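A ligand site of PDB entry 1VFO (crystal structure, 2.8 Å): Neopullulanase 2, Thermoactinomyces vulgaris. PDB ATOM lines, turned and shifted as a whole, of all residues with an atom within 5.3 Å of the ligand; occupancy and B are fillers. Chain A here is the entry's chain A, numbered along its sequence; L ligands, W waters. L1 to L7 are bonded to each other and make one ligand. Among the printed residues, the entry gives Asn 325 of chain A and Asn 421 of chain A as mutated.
The side-chain carboxylate (OD2) of Asp 465 lies within hydrogen-bond range of an oxygen (O1) of LG7 L7, 2.6 Å away.
An oxygen (O1) of LG4 L4 sits at hydrogen-bond distance from the side-chain amide oxygen (OD1) of Asn 421, 2.7 Å away.
The side-chain amide oxygen of Asn 325 sits close to an oxygen (O4) of LG4 L4, at 2.7 Å.
OE1 of Glu 354 lies within hydrogen-bond range of O1 of LG4 L4 (3.0 Å).
A ring nitrogen (NE2) of His 420 lies within hydrogen-bond range of an oxygen (O2) of LG4 L4, 3.0 Å away.
The guanidinium group of Arg 469 is in hydrogen-bond range of an oxygen (O2) of LG6 L6.
A ring nitrogen (NE2) of His 244 is in hydrogen-bond range of an oxygen (O5) of LG4 L4 (3.2 Å).
A ring nitrogen (ND1) of His 164 sits at hydrogen-bond distance from an oxygen (O1) of LG7 L7, at 3.4 Å.
Water W4 lies within hydrogen-bond range of an oxygen (O2) of LG7 L7 (2.8 Å) and the backbone carbonyl oxygen (O) of Asp 465 (3.1 Å).
Water W3 lies within hydrogen-bond range of a ring nitrogen (ND1) of His 164 (2.8 Å), the side-chain carboxylate (OD1) of Asp 465 (2.8 Å) and an oxygen (O1) of LG7 L7 (3.3 Å).
CD2 of His 202 touches O2 of LG6 L6, 3.7 Å away.
CD2 of Tyr 204 touches O1 of LG6 L6, 3.3 Å away.
Phe 286 touches the ligand.
CE of Met 293 touches O4 of LG6 L6 (3.6 Å).
CA of Val 326 touches O5 of LG2 L2, 3.5 Å away.
Trp 356 touches the ligand.
Hydrophobic or aromatic side chains that line the ligand: His 164, His 202, Tyr 204, His 244, Phe 286, Met 293, Val 326, Trp 356 and His 420.
Of the 19 residues printed, 14 come within 4 Å of the ligand.
OD1 of Asn 421 lies within hydrogen-bond range of NE2 of His 420 (3.3 Å).
The side-chain amide nitrogen (ND2) of Asn 421 lies close to the guanidinium group (NH2) of Arg 469 (3.4 Å).
The side-chain carboxylate (OE2) of Glu 354 sits close to the side-chain amide oxygen (OD1) of Asn 325 (3.1 Å).
N of Val 326 sits at hydrogen-bond distance from OE2 of Glu 354, at 3.3 Å.
The guanidinium group (NH1) of Arg 323 is in salt-bridge range of the side-chain carboxylate (OE1) of Glu 354 (3.4 Å).
O of His 420 is in hydrogen-bond range of NE of Arg 469 (2.9 Å).
The backbone NH of Phe 286 is in hydrogen-bond range of the backbone carbonyl oxygen of Met 293 (2.9 Å).
The backbone NH (N) of Tyr 204 lies within hydrogen-bond range of a ring nitrogen (ND1) of His 202.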
ATOM      1  N   HIS A 164     -21.277   5.718  22.222  1.00  0.00           N
ATOM      2  CA  HIS A 164     -21.391   4.266  22.163  1.00  0.00           C
ATOM      3  C   HIS A 164     -22.607   3.821  21.365  1.00  0.00           C
ATOM      4  O   HIS A 164     -22.676   2.667  20.943  1.00  0.00           O
ATOM      5  CB  HIS A 164     -21.473   3.688  23.580  1.00  0.00           C
ATOM      6  CG  HIS A 164     -20.186   3.749  24.330  1.00  0.00           C
ATOM      7  ND1 HIS A 164     -19.077   3.013  23.965  1.00  0.00           N
ATOM      8  CD2 HIS A 164     -19.819   4.471  25.418  1.00  0.00           C
ATOM      9  CE1 HIS A 164     -18.091   3.269  24.806  1.00  0.00           C
ATOM     10  NE2 HIS A 164     -18.513   4.149  25.693  1.00  0.00           N
ATOM     11  N   HIS A 201     -24.481  -0.772  16.675  1.00  0.00           N
ATOM     12  CA  HIS A 201     -23.721  -0.174  15.582  1.00  0.00           C
ATOM     13  C   HIS A 201     -22.483  -0.982  15.259  1.00  0.00           C
ATOM     14  O   HIS A 201     -21.853  -0.777  14.214  1.00  0.00           O
ATOM     15  CB  HIS A 201     -23.321   1.279  15.911  1.00  0.00           C
ATOM     16  CG  HIS A 201     -22.078   1.405  16.733  1.00  0.00           C
ATOM     17  ND1 HIS A 201     -22.065   1.267  18.099  1.00  0.00           N
ATOM     18  CD2 HIS A 201     -20.796   1.675  16.367  1.00  0.00           C
ATOM     19  CE1 HIS A 201     -20.840   1.455  18.552  1.00  0.00           C
ATOM     20  NE2 HIS A 201     -20.047   1.701  17.518  1.00  0.00           N
ATOM     21  N   HIS A 202     -22.112  -1.899  16.155  1.00  0.00           N
ATOM     22  CA  HIS A 202     -20.949  -2.767  15.957  1.00  0.00           C
ATOM     23  C   HIS A 202     -21.431  -4.121  15.454  1.00  0.00           C
ATOM     24  O   HIS A 202     -20.737  -4.815  14.718  1.00  0.00           O
ATOM     25  CB  HIS A 202     -20.154  -2.904  17.269  1.00  0.00           C
ATOM     26  CG  HIS A 202     -20.997  -3.260  18.449  1.00  0.00           C
ATOM     27  ND1 HIS A 202     -21.530  -4.521  18.633  1.00  0.00           N
ATOM     28  CD2 HIS A 202     -21.388  -2.525  19.524  1.00  0.00           C
ATOM     29  CE1 HIS A 202     -22.217  -4.542  19.764  1.00  0.00           C
ATOM     30  NE2 HIS A 202     -22.147  -3.353  20.326  1.00  0.00           N
ATOM     31  N   TYR A 204     -21.971  -7.105  16.975  1.00  0.00           N
ATOM     32  CA  TYR A 204     -21.320  -8.317  17.454  1.00  0.00           C
ATOM     33  C   TYR A 204     -22.359  -9.067  18.280  1.00  0.00           C
ATOM     34  O   TYR A 204     -22.071 -10.138  18.823  1.00  0.00           O
ATOM     35  CB  TYR A 204     -20.098  -7.984  18.315  1.00  0.00           C
ATOM     36  CG  TYR A 204     -18.809  -7.729  17.541  1.00  0.00           C
ATOM     37  CD1 TYR A 204     -17.996  -8.786  17.104  1.00  0.00           C
ATOM     38  CD2 TYR A 204     -18.396  -6.422  17.237  1.00  0.00           C
ATOM     39  CE1 TYR A 204     -16.811  -8.551  16.397  1.00  0.00           C
ATOM     40  CE2 TYR A 204     -17.212  -6.178  16.531  1.00  0.00           C
ATOM     41  CZ  TYR A 204     -16.417  -7.246  16.106  1.00  0.00           C
ATOM     42  OH  TYR A 204     -15.281  -7.004  15.362  1.00  0.00           O
ATOM     43  N   VAL A 241     -18.845 -14.525  14.390  1.00  0.00           N
ATOM     44  CA  VAL A 241     -19.043 -14.329  15.814  1.00  0.00           C
ATOM     45  C   VAL A 241     -19.772 -15.614  16.255  1.00  0.00           C
ATOM     46  O   VAL A 241     -20.988 -15.630  16.392  1.00  0.00           O
ATOM     47  CB  VAL A 241     -19.923 -13.081  16.104  1.00  0.00           C
ATOM     48  CG1 VAL A 241     -19.988 -12.797  17.608  1.00  0.00           C
ATOM     49  CG2 VAL A 241     -19.334 -11.887  15.386  1.00  0.00           C
ATOM     50  N   HIS A 244     -20.654 -16.350  20.751  1.00  0.00           N
ATOM     51  CA  HIS A 244     -21.906 -15.924  21.346  1.00  0.00           C
ATOM     52  C   HIS A 244     -22.838 -15.356  20.301  1.00  0.00           C
ATOM     53  O   HIS A 244     -22.431 -14.965  19.206  1.00  0.00           O
ATOM     54  CB  HIS A 244     -21.647 -14.889  22.433  1.00  0.00           C
ATOM     55  CG  HIS A 244     -20.706 -13.810  22.023  1.00  0.00           C
ATOM     56  ND1 HIS A 244     -21.124 -12.545  21.676  1.00  0.00           N
ATOM     57  CD2 HIS A 244     -19.358 -13.812  21.855  1.00  0.00           C
ATOM     58  CE1 HIS A 244     -20.088 -11.811  21.314  1.00  0.00           C
ATOM     59  NE2 HIS A 244     -19.003 -12.566  21.413  1.00  0.00           N
ATOM     60  N   PHE A 286     -20.754 -13.321  26.849  1.00  0.00           N
ATOM     61  CA  PHE A 286     -19.413 -12.896  26.504  1.00  0.00           C
ATOM     62  C   PHE A 286     -18.968 -11.969  27.639  1.00  0.00           C
ATOM     63  O   PHE A 286     -19.751 -11.163  28.130  1.00  0.00           O
ATOM     64  CB  PHE A 286     -19.424 -12.128  25.176  1.00  0.00           C
ATOM     65  CG  PHE A 286     -18.241 -11.229  24.987  1.00  0.00           C
ATOM     66  CD1 PHE A 286     -18.313  -9.881  25.313  1.00  0.00           C
ATOM     67  CD2 PHE A 286     -17.020 -11.744  24.562  1.00  0.00           C
ATOM     68  CE1 PHE A 286     -17.199  -9.061  25.217  1.00  0.00           C
ATOM     69  CE2 PHE A 286     -15.892 -10.923  24.462  1.00  0.00           C
ATOM     70  CZ  PHE A 286     -15.991  -9.587  24.796  1.00  0.00           C
ATOM     71  N   VAL A 290     -23.085  -9.250  30.204  1.00  0.00           N
ATOM     72  CA  VAL A 290     -23.370  -8.536  28.963  1.00  0.00           C
ATOM     73  C   VAL A 290     -24.602  -9.230  28.366  1.00  0.00           C
ATOM     74  O   VAL A 290     -24.493 -10.053  27.461  1.00  0.00           O
ATOM     75  CB  VAL A 290     -22.170  -8.611  27.990  1.00  0.00           C
ATOM     76  CG1 VAL A 290     -22.425  -7.755  26.764  1.00  0.00           C
ATOM     77  CG2 VAL A 290     -20.921  -8.141  28.705  1.00  0.00           C
ATOM     78  N   MET A 293     -25.253 -10.389  24.820  1.00  0.00           N
ATOM     79  CA  MET A 293     -24.448 -11.430  24.208  1.00  0.00           C
ATOM     80  C   MET A 293     -24.362 -12.774  24.940  1.00  0.00           C
ATOM     81  O   MET A 293     -23.364 -13.073  25.608  1.00  0.00           O
ATOM     82  CB  MET A 293     -23.024 -10.903  23.973  1.00  0.00           C
ATOM     83  CG  MET A 293     -22.974  -9.579  23.246  1.00  0.00           C
ATOM     84  SD  MET A 293     -21.291  -8.976  23.135  1.00  0.00           S
ATOM     85  CE  MET A 293     -21.207  -8.507  21.391  1.00  0.00           C
ATOM     86  N   ARG A 323     -12.571 -14.257  10.019  1.00  0.00           N
ATOM     87  CA  ARG A 323     -11.754 -13.783  11.127  1.00  0.00           C
ATOM     88  C   ARG A 323     -12.634 -14.301  12.263  1.00  0.00           C
ATOM     89  O   ARG A 323     -13.807 -13.951  12.348  1.00  0.00           O
ATOM     90  CB  ARG A 323     -11.676 -12.252  11.138  1.00  0.00           C
ATOM     91  CG  ARG A 323     -10.569 -11.648  12.014  1.00  0.00           C
ATOM     92  CD  ARG A 323     -10.652 -12.067  13.500  1.00  0.00           C
ATOM     93  NE  ARG A 323     -11.708 -11.412  14.277  1.00  0.00           N
ATOM     94  CZ  ARG A 323     -11.713 -10.120  14.612  1.00  0.00           C
ATOM     95  NH1 ARG A 323     -12.715  -9.618  15.326  1.00  0.00           N
ATOM     96  NH2 ARG A 323     -10.721  -9.328  14.219  1.00  0.00           N
ATOM     97  N   ASN A 325     -13.899 -14.187  15.725  1.00  0.00           N
ATOM     98  CA  ASN A 325     -14.027 -13.366  16.916  1.00  0.00           C
ATOM     99  C   ASN A 325     -14.137 -14.212  18.184  1.00  0.00           C
ATOM    100  O   ASN A 325     -14.927 -15.156  18.241  1.00  0.00           O
ATOM    101  CB  ASN A 325     -15.254 -12.469  16.751  1.00  0.00           C
ATOM    102  CG  ASN A 325     -15.571 -11.674  17.997  1.00  0.00           C
ATOM    103  OD1 ASN A 325     -14.749 -10.886  18.458  1.00  0.00           O
ATOM    104  ND2 ASN A 325     -16.761 -11.884  18.543  1.00  0.00           N
ATOM    105  N   VAL A 326     -13.358 -13.867  19.204  1.00  0.00           N
ATOM    106  CA  VAL A 326     -13.339 -14.594  20.494  1.00  0.00           C
ATOM    107  C   VAL A 326     -13.191 -16.099  20.254  1.00  0.00           C
ATOM    108  O   VAL A 326     -13.856 -16.905  20.904  1.00  0.00           O
ATOM    109  CB  VAL A 326     -14.664 -14.381  21.307  1.00  0.00           C
ATOM    110  CG1 VAL A 326     -14.408 -14.655  22.783  1.00  0.00           C
ATOM    111  CG2 VAL A 326     -15.219 -12.981  21.112  1.00  0.00           C
ATOM    112  N   ASN A 328     -10.727 -18.216  20.976  1.00  0.00           N
ATOM    113  CA  ASN A 328     -10.149 -19.042  22.027  1.00  0.00           C
ATOM    114  C   ASN A 328     -11.148 -19.515  23.044  1.00  0.00           C
ATOM    115  O   ASN A 328     -10.801 -20.292  23.927  1.00  0.00           O
ATOM    116  CB  ASN A 328      -9.000 -18.308  22.730  1.00  0.00           C
ATOM    117  CG  ASN A 328      -9.389 -16.950  23.238  1.00  0.00           C
ATOM    118  OD1 ASN A 328     -10.256 -16.293  22.669  1.00  0.00           O
ATOM    119  ND2 ASN A 328      -8.757 -16.519  24.311  1.00  0.00           N
ATOM    120  N   GLU A 354      -8.600 -14.683  16.379  1.00  0.00           N
ATOM    121  CA  GLU A 354      -8.428 -13.516  17.258  1.00  0.00           C
ATOM    122  C   GLU A 354      -8.200 -13.991  18.681  1.00  0.00           C
ATOM    123  O   GLU A 354      -9.162 -14.160  19.433  1.00  0.00           O
ATOM    124  CB  GLU A 354      -9.681 -12.647  17.224  1.00  0.00           C
ATOM    125  CG  GLU A 354      -9.429 -11.195  17.575  1.00  0.00           C
ATOM    126  CD  GLU A 354     -10.682 -10.442  18.012  1.00  0.00           C
ATOM    127  OE1 GLU A 354     -10.651  -9.203  17.952  1.00  0.00           O
ATOM    128  OE2 GLU A 354     -11.685 -11.094  18.409  1.00  0.00           O
ATOM    129  N   TRP A 356      -5.804 -13.292  22.216  1.00  0.00           N
ATOM    130  CA  TRP A 356      -4.946 -12.306  22.861  1.00  0.00           C
ATOM    131  C   TRP A 356      -3.961 -12.900  23.876  1.00  0.00           C
ATOM    132  O   TRP A 356      -3.821 -12.386  24.984  1.00  0.00           O
ATOM    133  CB  TRP A 356      -5.838 -11.252  23.505  1.00  0.00           C
ATOM    134  CG  TRP A 356      -5.174  -9.937  23.784  1.00  0.00           C
ATOM    135  CD1 TRP A 356      -4.523  -9.134  22.888  1.00  0.00           C
ATOM    136  CD2 TRP A 356      -5.115  -9.265  25.043  1.00  0.00           C
ATOM    137  NE1 TRP A 356      -4.065  -7.998  23.520  1.00  0.00           N
ATOM    138  CE2 TRP A 356      -4.412  -8.051  24.845  1.00  0.00           C
ATOM    139  CE3 TRP A 356      -5.598  -9.567  26.331  1.00  0.00           C
ATOM    140  CZ2 TRP A 356      -4.172  -7.146  25.877  1.00  0.00           C
ATOM    141  CZ3 TRP A 356      -5.354  -8.662  27.355  1.00  0.00           C
ATOM    142  CH2 TRP A 356      -4.653  -7.467  27.120  1.00  0.00           C
ATOM    143  N   HIS A 420     -10.739  -1.187  15.812  1.00  0.00           N
ATOM    144  CA  HIS A 420     -11.981  -0.534  16.259  1.00  0.00           C
ATOM    145  C   HIS A 420     -12.075  -0.684  17.759  1.00  0.00           C
ATOM    146  O   HIS A 420     -13.137  -0.454  18.340  1.00  0.00           O
ATOM    147  CB  HIS A 420     -13.200  -1.197  15.636  1.00  0.00           C
ATOM    148  CG  HIS A 420     -13.264  -2.674  15.842  1.00  0.00           C
ATOM    149  ND1 HIS A 420     -12.528  -3.565  15.091  1.00  0.00           N
ATOM    150  CD2 HIS A 420     -13.982  -3.421  16.707  1.00  0.00           C
ATOM    151  CE1 HIS A 420     -12.788  -4.803  15.483  1.00  0.00           C
ATOM    152  NE2 HIS A 420     -13.668  -4.743  16.458  1.00  0.00           N
ATOM    153  N   ASN A 421     -10.974  -1.074  18.374  1.00  0.00           N
ATOM    154  CA  ASN A 421     -10.907  -1.260  19.811  1.00  0.00           C
ATOM    155  C   ASN A 421      -9.781  -0.485  20.448  1.00  0.00           C
ATOM    156  O   ASN A 421      -9.504  -0.646  21.625  1.00  0.00           O
ATOM    157  CB  ASN A 421     -10.742  -2.745  20.141  1.00  0.00           C
ATOM    158  CG  ASN A 421     -11.992  -3.542  19.880  1.00  0.00           C
ATOM    159  OD1 ASN A 421     -11.926  -4.621  19.308  1.00  0.00           O
ATOM    160  ND2 ASN A 421     -13.133  -3.011  20.303  1.00  0.00           N
ATOM    161  N   ASP A 465     -12.331   3.318  21.542  1.00  0.00           N
ATOM    162  CA  ASP A 465     -13.769   3.145  21.351  1.00  0.00           C
ATOM    163  C   ASP A 465     -14.556   4.087  22.273  1.00  0.00           C
ATOM    164  O   ASP A 465     -14.364   4.089  23.484  1.00  0.00           O
ATOM    165  CB  ASP A 465     -14.143   1.682  21.641  1.00  0.00           C
ATOM    166  CG  ASP A 465     -15.582   1.354  21.301  1.00  0.00           C
ATOM    167  OD1 ASP A 465     -16.292   2.232  20.777  1.00  0.00           O
ATOM    168  OD2 ASP A 465     -16.004   0.199  21.565  1.00  0.00           O
ATOM    169  N   ARG A 469     -13.797   5.137  16.012  1.00  0.00           N
ATOM    170  CA  ARG A 469     -14.790   4.735  15.030  1.00  0.00           C
ATOM    171  C   ARG A 469     -15.475   5.979  14.445  1.00  0.00           C
ATOM    172  O   ARG A 469     -16.698   6.049  14.378  1.00  0.00           O
ATOM    173  CB  ARG A 469     -15.826   3.801  15.685  1.00  0.00           C
ATOM    174  CG  ARG A 469     -15.237   2.576  16.402  1.00  0.00           C
ATOM    175  CD  ARG A 469     -16.313   1.728  17.098  1.00  0.00           C
ATOM    176  NE  ARG A 469     -15.744   0.525  17.704  1.00  0.00           N
ATOM    177  CZ  ARG A 469     -16.415  -0.365  18.458  1.00  0.00           C
ATOM    178  NH1 ARG A 469     -17.707  -0.201  18.714  1.00  0.00           N
ATOM    179  NH2 ARG A 469     -15.776  -1.417  18.942  1.00  0.00           N
HETATM  180  C1  LIG L   1      -8.673  -6.475  28.227  1.00  0.00           C
HETATM  181  C2  LIG L   1      -7.838  -5.999  27.051  1.00  0.00           C
HETATM  182  C3  LIG L   1      -8.532  -6.316  25.725  1.00  0.00           C
HETATM  183  C4  LIG L   1      -9.009  -7.764  25.641  1.00  0.00           C
HETATM  184  C5  LIG L   1      -9.786  -8.148  26.889  1.00  0.00           C
HETATM  185  C6  LIG L   1     -10.094  -9.627  26.916  1.00  0.00           C
HETATM  186  O1  LIG L   1      -7.682  -4.596  27.163  1.00  0.00           O
HETATM  187  O2  LIG L   1      -7.641  -6.051  24.656  1.00  0.00           O
HETATM  188  O3  LIG L   1      -9.852  -7.918  24.486  1.00  0.00           O
HETATM  189  O4  LIG L   1      -9.009  -7.849  28.065  1.00  0.00           O
HETATM  190  O5  LIG L   1      -8.929 -10.390  27.161  1.00  0.00           O
HETATM  191  C1  LG2 L   2      -9.457  -8.899  23.576  1.00  0.00           C
HETATM  192  C2  LG2 L   2      -9.258  -8.284  22.191  1.00  0.00           C
HETATM  193  C3  LG2 L   2     -10.592  -7.764  21.654  1.00  0.00           C
HETATM  194  C4  LG2 L   2     -11.663  -8.868  21.660  1.00  0.00           C
HETATM  195  C5  LG2 L   2     -11.731  -9.554  23.042  1.00  0.00           C
HETATM  196  C6  LG2 L   2     -12.546 -10.828  22.993  1.00  0.00           C
HETATM  197  O1  LG2 L   2      -8.337  -7.204  22.295  1.00  0.00           O
HETATM  198  O2  LG2 L   2     -10.406  -7.292  20.330  1.00  0.00           O
HETATM  199  O3  LG2 L   2     -12.935  -8.262  21.357  1.00  0.00           O
HETATM  200  O4  LG2 L   2     -10.413  -9.952  23.490  1.00  0.00           O
HETATM  201  O5  LG2 L   2     -12.048 -11.709  21.987  1.00  0.00           O
HETATM  202  C1  LG3 L   3     -11.705  -3.015  30.903  1.00  0.00           C
HETATM  203  C2  LG3 L   3     -10.273  -2.632  30.502  1.00  0.00           C
HETATM  204  C3  LG3 L   3      -9.886  -3.412  29.250  1.00  0.00           C
HETATM  205  C4  LG3 L   3      -9.999  -4.925  29.529  1.00  0.00           C
HETATM  206  C5  LG3 L   3     -11.394  -5.260  30.045  1.00  0.00           C
HETATM  207  C6  LG3 L   3     -11.523  -6.700  30.492  1.00  0.00           C
HETATM  208  O1  LG3 L   3     -10.197  -1.232  30.239  1.00  0.00           O
HETATM  209  O2  LG3 L   3      -8.569  -3.057  28.852  1.00  0.00           O
HETATM  210  O3  LG3 L   3      -9.791  -5.659  28.308  1.00  0.00           O
HETATM  211  O4  LG3 L   3     -11.755  -4.414  31.180  1.00  0.00           O
HETATM  212  O5  LG3 L   3     -10.264  -7.258  30.815  1.00  0.00           O
HETATM  213  C1  LG4 L   4     -13.659  -8.780  20.273  1.00  0.00           C
HETATM  214  C2  LG4 L   4     -13.909  -7.679  19.240  1.00  0.00           C
HETATM  215  C3  LG4 L   4     -14.727  -6.550  19.908  1.00  0.00           C
HETATM  216  C4  LG4 L   4     -16.028  -7.101  20.505  1.00  0.00           C
HETATM  217  C5  LG4 L   4     -15.774  -8.357  21.380  1.00  0.00           C
HETATM  218  C6  LG4 L   4     -17.044  -9.088  21.751  1.00  0.00           C
HETATM  219  O1  LG4 L   4     -12.679  -7.187  18.737  1.00  0.00           O
HETATM  220  O2  LG4 L   4     -15.020  -5.516  18.983  1.00  0.00           O
HETATM  221  O3  LG4 L   4     -16.623  -6.081  21.320  1.00  0.00           O
HETATM  222  O4  LG4 L   4     -14.919  -9.311  20.688  1.00  0.00           O
HETATM  223  O5  LG4 L   4     -17.554  -9.820  20.653  1.00  0.00           O
HETATM  224  C1  LG5 L   5     -16.495  -1.334  29.304  1.00  0.00           C
HETATM  225  C2  LG5 L   5     -15.454  -0.229  29.499  1.00  0.00           C
HETATM  226  C3  LG5 L   5     -14.044  -0.808  29.320  1.00  0.00           C
HETATM  227  C4  LG5 L   5     -13.822  -2.028  30.226  1.00  0.00           C
HETATM  228  C5  LG5 L   5     -14.956  -3.040  30.046  1.00  0.00           C
HETATM  229  C6  LG5 L   5     -14.878  -4.174  31.062  1.00  0.00           C
HETATM  230  O1  LG5 L   5     -15.657   0.812  28.555  1.00  0.00           O
HETATM  231  O2  LG5 L   5     -13.075   0.188  29.615  1.00  0.00           O
HETATM  232  O3  LG5 L   5     -12.582  -2.644  29.861  1.00  0.00           O
HETATM  233  O4  LG5 L   5     -16.239  -2.401  30.218  1.00  0.00           O
HETATM  234  O5  LG5 L   5     -16.151  -4.470  31.602  1.00  0.00           O
HETATM  235  C1  LG6 L   6     -17.976  -5.814  21.095  1.00  0.00           C
HETATM  236  C2  LG6 L   6     -18.152  -4.383  20.538  1.00  0.00           C
HETATM  237  C3  LG6 L   6     -17.788  -3.349  21.602  1.00  0.00           C
HETATM  238  C4  LG6 L   6     -18.551  -3.593  22.914  1.00  0.00           C
HETATM  239  C5  LG6 L   6     -18.400  -5.062  23.352  1.00  0.00           C
HETATM  240  C6  LG6 L   6     -19.215  -5.458  24.567  1.00  0.00           C
HETATM  241  O1  LG6 L   6     -17.309  -4.209  19.401  1.00  0.00           O
HETATM  242  O2  LG6 L   6     -18.082  -2.049  21.108  1.00  0.00           O
HETATM  243  O3  LG6 L   6     -17.989  -2.733  23.924  1.00  0.00           O
HETATM  244  O4  LG6 L   6     -18.763  -5.965  22.275  1.00  0.00           O
HETATM  245  O5  LG6 L   6     -20.506  -4.862  24.549  1.00  0.00           O
HETATM  246  C1  LG7 L   7     -18.855  -1.838  24.559  1.00  0.00           C
HETATM  247  C2  LG7 L   7     -18.139  -0.509  24.845  1.00  0.00           C
HETATM  248  C3  LG7 L   7     -17.040  -0.724  25.883  1.00  0.00           C
HETATM  249  C4  LG7 L   7     -17.595  -1.392  27.150  1.00  0.00           C
HETATM  250  C5  LG7 L   7     -18.417  -2.646  26.801  1.00  0.00           C
HETATM  251  C6  LG7 L   7     -19.167  -3.236  27.980  1.00  0.00           C
HETATM  252  O1  LG7 L   7     -17.572   0.017  23.653  1.00  0.00           O
HETATM  253  O2  LG7 L   7     -16.436   0.515  26.215  1.00  0.00           O
HETATM  254  O3  LG7 L   7     -16.476  -1.768  27.981  1.00  0.00           O
HETATM  255  O4  LG7 L   7     -19.392  -2.363  25.779  1.00  0.00           O
HETATM  256  O5  LG7 L   7     -20.323  -3.951  27.559  1.00  0.00           O
HETATM  257  O   HOH W   1     -11.963   1.701  27.494  1.00  0.00           O
HETATM  258  O   HOH W   2     -17.063  -7.005  31.255  1.00  0.00           O
HETATM  259  O   HOH W   3     -19.054   1.951  21.409  1.00  0.00           O
HETATM  260  O   HOH W   4     -13.961   1.568  25.279  1.00  0.00           O
